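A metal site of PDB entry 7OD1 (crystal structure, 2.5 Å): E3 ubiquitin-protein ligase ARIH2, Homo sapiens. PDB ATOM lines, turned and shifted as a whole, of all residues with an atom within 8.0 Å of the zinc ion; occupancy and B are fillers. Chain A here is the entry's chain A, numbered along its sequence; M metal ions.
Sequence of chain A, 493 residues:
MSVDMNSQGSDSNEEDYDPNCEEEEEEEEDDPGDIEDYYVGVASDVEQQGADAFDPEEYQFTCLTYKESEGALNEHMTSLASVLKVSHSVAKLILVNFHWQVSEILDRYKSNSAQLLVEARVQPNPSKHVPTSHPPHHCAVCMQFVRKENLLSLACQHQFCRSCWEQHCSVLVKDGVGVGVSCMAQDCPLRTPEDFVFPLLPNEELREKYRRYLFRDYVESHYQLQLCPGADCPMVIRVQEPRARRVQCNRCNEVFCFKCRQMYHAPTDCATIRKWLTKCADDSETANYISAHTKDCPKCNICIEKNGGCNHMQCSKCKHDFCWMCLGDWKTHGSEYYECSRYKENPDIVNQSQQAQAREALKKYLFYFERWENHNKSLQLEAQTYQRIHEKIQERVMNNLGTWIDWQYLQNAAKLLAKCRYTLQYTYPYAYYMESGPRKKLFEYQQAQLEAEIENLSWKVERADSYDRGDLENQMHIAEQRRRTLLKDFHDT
Merely in contact with the zinc ion: Val 141 (3.97 Å). Of the 20 residues printed, 5 come within 4 Å of the zinc ion.
The zinc ion is bound by SG of Cys 164, SG of Cys 142, SG of Cys 161 and SG of Cys 139.
The side-chain sulfur (SG) of Cys 139 sits close to the backbone NH (N) of Val 141 (3.8 Å). The backbone NH (N) of Cys 139 lies within hydrogen-bond range of the backbone carbonyl oxygen (O) of Gln 144.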
ATOM      1  N   HIS A 138       0.162   0.533   7.341  1.00  0.00           N
ATOM      2  CA  HIS A 138       0.886   0.149   8.547  1.00  0.00           C
ATOM      3  C   HIS A 138       0.102   0.680   9.737  1.00  0.00           C
ATOM      4  O   HIS A 138       0.142   1.881  10.012  1.00  0.00           O
ATOM      5  CB  HIS A 138       2.310   0.703   8.521  1.00  0.00           C
ATOM      6  CG  HIS A 138       3.058   0.517   9.816  1.00  0.00           C
ATOM      7  ND1 HIS A 138       3.457   1.585  10.595  1.00  0.00           N
ATOM      8  CD2 HIS A 138       3.478  -0.599  10.453  1.00  0.00           C
ATOM      9  CE1 HIS A 138       4.089   1.119  11.668  1.00  0.00           C
ATOM     10  NE2 HIS A 138       4.107  -0.192  11.599  1.00  0.00           N
ATOM     11  N   CYS A 139      -0.604  -0.198  10.438  1.00  0.00           N
ATOM     12  CA  CYS A 139      -1.402   0.215  11.587  1.00  0.00           C
ATOM     13  C   CYS A 139      -0.486   0.478  12.775  1.00  0.00           C
ATOM     14  O   CYS A 139       0.359  -0.352  13.117  1.00  0.00           O
ATOM     15  CB  CYS A 139      -2.436  -0.859  11.938  1.00  0.00           C
ATOM     16  SG  CYS A 139      -3.475  -0.428  13.342  1.00  0.00           S
ATOM     17  N   ALA A 140      -0.665   1.644  13.401  1.00  0.00           N
ATOM     18  CA  ALA A 140       0.262   2.093  14.434  1.00  0.00           C
ATOM     19  C   ALA A 140       0.146   1.317  15.739  1.00  0.00           C
ATOM     20  O   ALA A 140       1.003   1.489  16.612  1.00  0.00           O
ATOM     21  CB  ALA A 140       0.043   3.590  14.708  1.00  0.00           C
ATOM     22  N   VAL A 141      -0.887   0.482  15.904  1.00  0.00           N
ATOM     23  CA  VAL A 141      -1.072  -0.257  17.146  1.00  0.00           C
ATOM     24  C   VAL A 141      -0.853  -1.763  16.983  1.00  0.00           C
ATOM     25  O   VAL A 141      -0.561  -2.435  17.989  1.00  0.00           O
ATOM     26  CB  VAL A 141      -2.455   0.022  17.761  1.00  0.00           C
ATOM     27  CG1 VAL A 141      -2.779   1.510  17.697  1.00  0.00           C
ATOM     28  CG2 VAL A 141      -3.529  -0.783  17.068  1.00  0.00           C
ATOM     29  N   CYS A 142      -0.969  -2.311  15.768  1.00  0.00           N
ATOM     30  CA  CYS A 142      -0.643  -3.702  15.523  1.00  0.00           C
ATOM     31  C   CYS A 142       0.609  -3.889  14.674  1.00  0.00           C
ATOM     32  O   CYS A 142       1.064  -5.021  14.511  1.00  0.00           O
ATOM     33  CB  CYS A 142      -1.832  -4.433  14.874  1.00  0.00           C
ATOM     34  SG  CYS A 142      -2.263  -3.930  13.185  1.00  0.00           S
ATOM     35  N   MET A 143       1.170  -2.796  14.147  1.00  0.00           N
ATOM     36  CA  MET A 143       2.440  -2.753  13.424  1.00  0.00           C
ATOM     37  C   MET A 143       2.444  -3.610  12.150  1.00  0.00           C
ATOM     38  O   MET A 143       3.492  -3.735  11.509  1.00  0.00           O
ATOM     39  CB  MET A 143       3.615  -3.160  14.315  1.00  0.00           C
ATOM     40  CG  MET A 143       4.577  -2.018  14.634  1.00  0.00           C
ATOM     41  SD  MET A 143       3.719  -0.522  15.149  1.00  0.00           S
ATOM     42  CE  MET A 143       3.154  -1.009  16.780  1.00  0.00           C
ATOM     43  N   GLN A 144       1.306  -4.170  11.768  1.00  0.00           N
ATOM     44  CA  GLN A 144       1.235  -5.000  10.574  1.00  0.00           C
ATOM     45  C   GLN A 144       0.847  -4.169   9.364  1.00  0.00           C
ATOM     46  O   GLN A 144       0.177  -3.149   9.482  1.00  0.00           O
ATOM     47  CB  GLN A 144       0.234  -6.138  10.770  1.00  0.00           C
ATOM     48  CG  GLN A 144       0.484  -6.987  12.006  1.00  0.00           C
ATOM     49  CD  GLN A 144      -0.559  -8.071  12.187  1.00  0.00           C
ATOM     50  OE1 GLN A 144      -0.880  -8.810  11.249  1.00  0.00           O
ATOM     51  NE2 GLN A 144      -1.103  -8.188  13.399  1.00  0.00           N
ATOM     52  N   PHE A 145       1.282  -4.630   8.194  1.00  0.00           N
ATOM     53  CA  PHE A 145       0.919  -3.976   6.944  1.00  0.00           C
ATOM     54  C   PHE A 145      -0.458  -4.446   6.502  1.00  0.00           C
ATOM     55  O   PHE A 145      -0.800  -5.622   6.633  1.00  0.00           O
ATOM     56  CB  PHE A 145       1.973  -4.265   5.865  1.00  0.00           C
ATOM     57  CG  PHE A 145       3.376  -3.917   6.280  1.00  0.00           C
ATOM     58  CD1 PHE A 145       4.108  -4.781   7.076  1.00  0.00           C
ATOM     59  CD2 PHE A 145       3.954  -2.720   5.882  1.00  0.00           C
ATOM     60  CE1 PHE A 145       5.407  -4.455   7.456  1.00  0.00           C
ATOM     61  CE2 PHE A 145       5.244  -2.397   6.257  1.00  0.00           C
ATOM     62  CZ  PHE A 145       5.968  -3.263   7.048  1.00  0.00           C
ATOM     63  N   VAL A 146      -1.257  -3.516   5.985  1.00  0.00           N
ATOM     64  CA  VAL A 146      -2.658  -3.771   5.669  1.00  0.00           C
ATOM     65  C   VAL A 146      -2.989  -3.156   4.317  1.00  0.00           C
ATOM     66  O   VAL A 146      -2.193  -2.425   3.718  1.00  0.00           O
ATOM     67  CB  VAL A 146      -3.604  -3.206   6.752  1.00  0.00           C
ATOM     68  CG1 VAL A 146      -3.483  -4.025   8.034  1.00  0.00           C
ATOM     69  CG2 VAL A 146      -3.308  -1.741   7.004  1.00  0.00           C
ATOM     70  N   ASN A 150      -8.764  -1.275   4.100  1.00  0.00           N
ATOM     71  CA  ASN A 150      -8.847  -1.706   5.490  1.00  0.00           C
ATOM     72  C   ASN A 150      -8.085  -0.779   6.430  1.00  0.00           C
ATOM     73  O   ASN A 150      -7.627  -1.218   7.485  1.00  0.00           O
ATOM     74  CB  ASN A 150      -8.325  -3.142   5.617  1.00  0.00           C
ATOM     75  CG  ASN A 150      -9.056  -4.110   4.706  1.00  0.00           C
ATOM     76  OD1 ASN A 150      -8.453  -4.998   4.110  1.00  0.00           O
ATOM     77  ND2 ASN A 150     -10.377  -3.944   4.606  1.00  0.00           N
ATOM     78  N   LEU A 151      -7.952   0.495   6.074  1.00  0.00           N
ATOM     79  CA  LEU A 151      -7.209   1.481   6.869  1.00  0.00           C
ATOM     80  C   LEU A 151      -8.122   2.684   7.057  1.00  0.00           C
ATOM     81  O   LEU A 151      -8.226   3.540   6.172  1.00  0.00           O
ATOM     82  CB  LEU A 151      -5.904   1.865   6.185  1.00  0.00           C
ATOM     83  CG  LEU A 151      -4.875   2.665   6.983  1.00  0.00           C
ATOM     84  CD1 LEU A 151      -4.396   1.863   8.183  1.00  0.00           C
ATOM     85  CD2 LEU A 151      -3.702   3.060   6.108  1.00  0.00           C
ATOM     86  N   GLN A 159      -4.711   7.192  10.856  1.00  0.00           N
ATOM     87  CA  GLN A 159      -5.163   5.959  10.214  1.00  0.00           C
ATOM     88  C   GLN A 159      -4.773   4.735  11.025  1.00  0.00           C
ATOM     89  O   GLN A 159      -3.660   4.627  11.534  1.00  0.00           O
ATOM     90  CB  GLN A 159      -4.587   5.860   8.796  1.00  0.00           C
ATOM     91  CG  GLN A 159      -5.469   6.480   7.736  1.00  0.00           C
ATOM     92  CD  GLN A 159      -4.679   7.165   6.641  1.00  0.00           C
ATOM     93  OE1 GLN A 159      -4.274   6.550   5.668  1.00  0.00           O
ATOM     94  NE2 GLN A 159      -4.444   8.471   6.808  1.00  0.00           N
ATOM     95  N   PHE A 160      -5.733   3.801  11.150  1.00  0.00           N
ATOM     96  CA  PHE A 160      -5.509   2.520  11.800  1.00  0.00           C
ATOM     97  C   PHE A 160      -6.279   1.455  11.031  1.00  0.00           C
ATOM     98  O   PHE A 160      -7.235   1.749  10.312  1.00  0.00           O
ATOM     99  CB  PHE A 160      -5.952   2.545  13.269  1.00  0.00           C
ATOM    100  CG  PHE A 160      -5.308   3.622  14.090  1.00  0.00           C
ATOM    101  CD1 PHE A 160      -5.889   4.876  14.184  1.00  0.00           C
ATOM    102  CD2 PHE A 160      -4.113   3.390  14.749  1.00  0.00           C
ATOM    103  CE1 PHE A 160      -5.295   5.877  14.943  1.00  0.00           C
ATOM    104  CE2 PHE A 160      -3.515   4.389  15.500  1.00  0.00           C
ATOM    105  CZ  PHE A 160      -4.108   5.633  15.601  1.00  0.00           C
ATOM    106  N   CYS A 161      -5.846   0.204  11.180  1.00  0.00           N
ATOM    107  CA  CYS A 161      -6.429  -0.866  10.396  1.00  0.00           C
ATOM    108  C   CYS A 161      -7.810  -1.249  10.937  1.00  0.00           C
ATOM    109  O   CYS A 161      -8.158  -0.965  12.082  1.00  0.00           O
ATOM    110  CB  CYS A 161      -5.508  -2.078  10.346  1.00  0.00           C
ATOM    111  SG  CYS A 161      -5.484  -3.125  11.813  1.00  0.00           S
ATOM    112  N   ARG A 162      -8.595  -1.913  10.078  1.00  0.00           N
ATOM    113  CA  ARG A 162      -9.995  -2.166  10.397  1.00  0.00           C
ATOM    114  C   ARG A 162     -10.137  -3.117  11.583  1.00  0.00           C
ATOM    115  O   ARG A 162     -11.015  -2.919  12.433  1.00  0.00           O
ATOM    116  CB  ARG A 162     -10.712  -2.742   9.177  1.00  0.00           C
ATOM    117  CG  ARG A 162     -12.191  -3.004   9.390  1.00  0.00           C
ATOM    118  CD  ARG A 162     -12.869  -3.478   8.110  1.00  0.00           C
ATOM    119  NE  ARG A 162     -12.840  -2.468   7.056  1.00  0.00           N
ATOM    120  CZ  ARG A 162     -13.694  -1.455   6.978  1.00  0.00           C
ATOM    121  NH1 ARG A 162     -14.656  -1.286   7.866  1.00  0.00           N
ATOM    122  NH2 ARG A 162     -13.581  -0.589   5.973  1.00  0.00           N
ATOM    123  N   SER A 163      -9.291  -4.142  11.660  1.00  0.00           N
ATOM    124  CA  SER A 163      -9.396  -5.104  12.763  1.00  0.00           C
ATOM    125  C   SER A 163      -9.177  -4.422  14.107  1.00  0.00           C
ATOM    126  O   SER A 163      -9.890  -4.706  15.073  1.00  0.00           O
ATOM    127  CB  SER A 163      -8.379  -6.235  12.563  1.00  0.00           C
ATOM    128  OG  SER A 163      -8.679  -6.978  11.398  1.00  0.00           O
ATOM    129  N   CYS A 164      -8.200  -3.512  14.176  1.00  0.00           N
ATOM    130  CA  CYS A 164      -7.946  -2.830  15.434  1.00  0.00           C
ATOM    131  C   CYS A 164      -9.039  -1.824  15.772  1.00  0.00           C
ATOM    132  O   CYS A 164      -9.358  -1.639  16.958  1.00  0.00           O
ATOM    133  CB  CYS A 164      -6.578  -2.144  15.378  1.00  0.00           C
ATOM    134  SG  CYS A 164      -5.194  -3.306  15.531  1.00  0.00           S
ATOM    135  N   TRP A 165      -9.651  -1.188  14.768  1.00  0.00           N
ATOM    136  CA  TRP A 165     -10.821  -0.364  15.018  1.00  0.00           C
ATOM    137  C   TRP A 165     -11.965  -1.193  15.592  1.00  0.00           C
ATOM    138  O   TRP A 165     -12.642  -0.765  16.536  1.00  0.00           O
ATOM    139  CB  TRP A 165     -11.269   0.332  13.730  1.00  0.00           C
ATOM    140  CG  TRP A 165     -10.642   1.681  13.506  1.00  0.00           C
ATOM    141  CD1 TRP A 165      -9.785   2.024  12.507  1.00  0.00           C
ATOM    142  CD2 TRP A 165     -10.853   2.860  14.290  1.00  0.00           C
ATOM    143  NE1 TRP A 165      -9.438   3.351  12.631  1.00  0.00           N
ATOM    144  CE2 TRP A 165     -10.082   3.888  13.714  1.00  0.00           C
ATOM    145  CE3 TRP A 165     -11.613   3.158  15.428  1.00  0.00           C
ATOM    146  CZ2 TRP A 165     -10.047   5.181  14.228  1.00  0.00           C
ATOM    147  CZ3 TRP A 165     -11.586   4.439  15.940  1.00  0.00           C
ATOM    148  CH2 TRP A 165     -10.806   5.441  15.341  1.00  0.00           C
ATOM    149  N   GLN A 167     -11.711  -4.029  17.278  1.00  0.00           N
ATOM    150  CA  GLN A 167     -11.356  -4.418  18.641  1.00  0.00           C
ATOM    151  C   GLN A 167     -11.538  -3.253  19.613  1.00  0.00           C
ATOM    152  O   GLN A 167     -12.082  -3.427  20.707  1.00  0.00           O
ATOM    153  CB  GLN A 167      -9.911  -4.927  18.669  1.00  0.00           C
ATOM    154  CG  GLN A 167      -9.556  -5.747  19.892  1.00  0.00           C
ATOM    155  CD  GLN A 167      -8.610  -5.029  20.838  1.00  0.00           C
ATOM    156  OE1 GLN A 167      -7.721  -4.304  20.394  1.00  0.00           O
ATOM    157  NE2 GLN A 167      -8.800  -5.218  22.129  1.00  0.00           N
ATOM    158  N   MET A 184      -7.978   6.418  18.348  1.00  0.00           N
ATOM    159  CA  MET A 184      -7.045   5.517  19.012  1.00  0.00           C
ATOM    160  C   MET A 184      -5.679   6.139  19.269  1.00  0.00           C
ATOM    161  O   MET A 184      -4.860   5.524  19.953  1.00  0.00           O
ATOM    162  CB  MET A 184      -6.882   4.239  18.198  1.00  0.00           C
ATOM    163  CG  MET A 184      -8.184   3.681  17.642  1.00  0.00           C
ATOM    164  SD  MET A 184      -8.076   1.936  17.249  1.00  0.00           S
ATOM    165  CE  MET A 184      -7.070   1.336  18.607  1.00  0.00           C
HETATM  166 ZN    ZN M   1      -4.120  -2.629  13.606  1.00  0.00          ZN
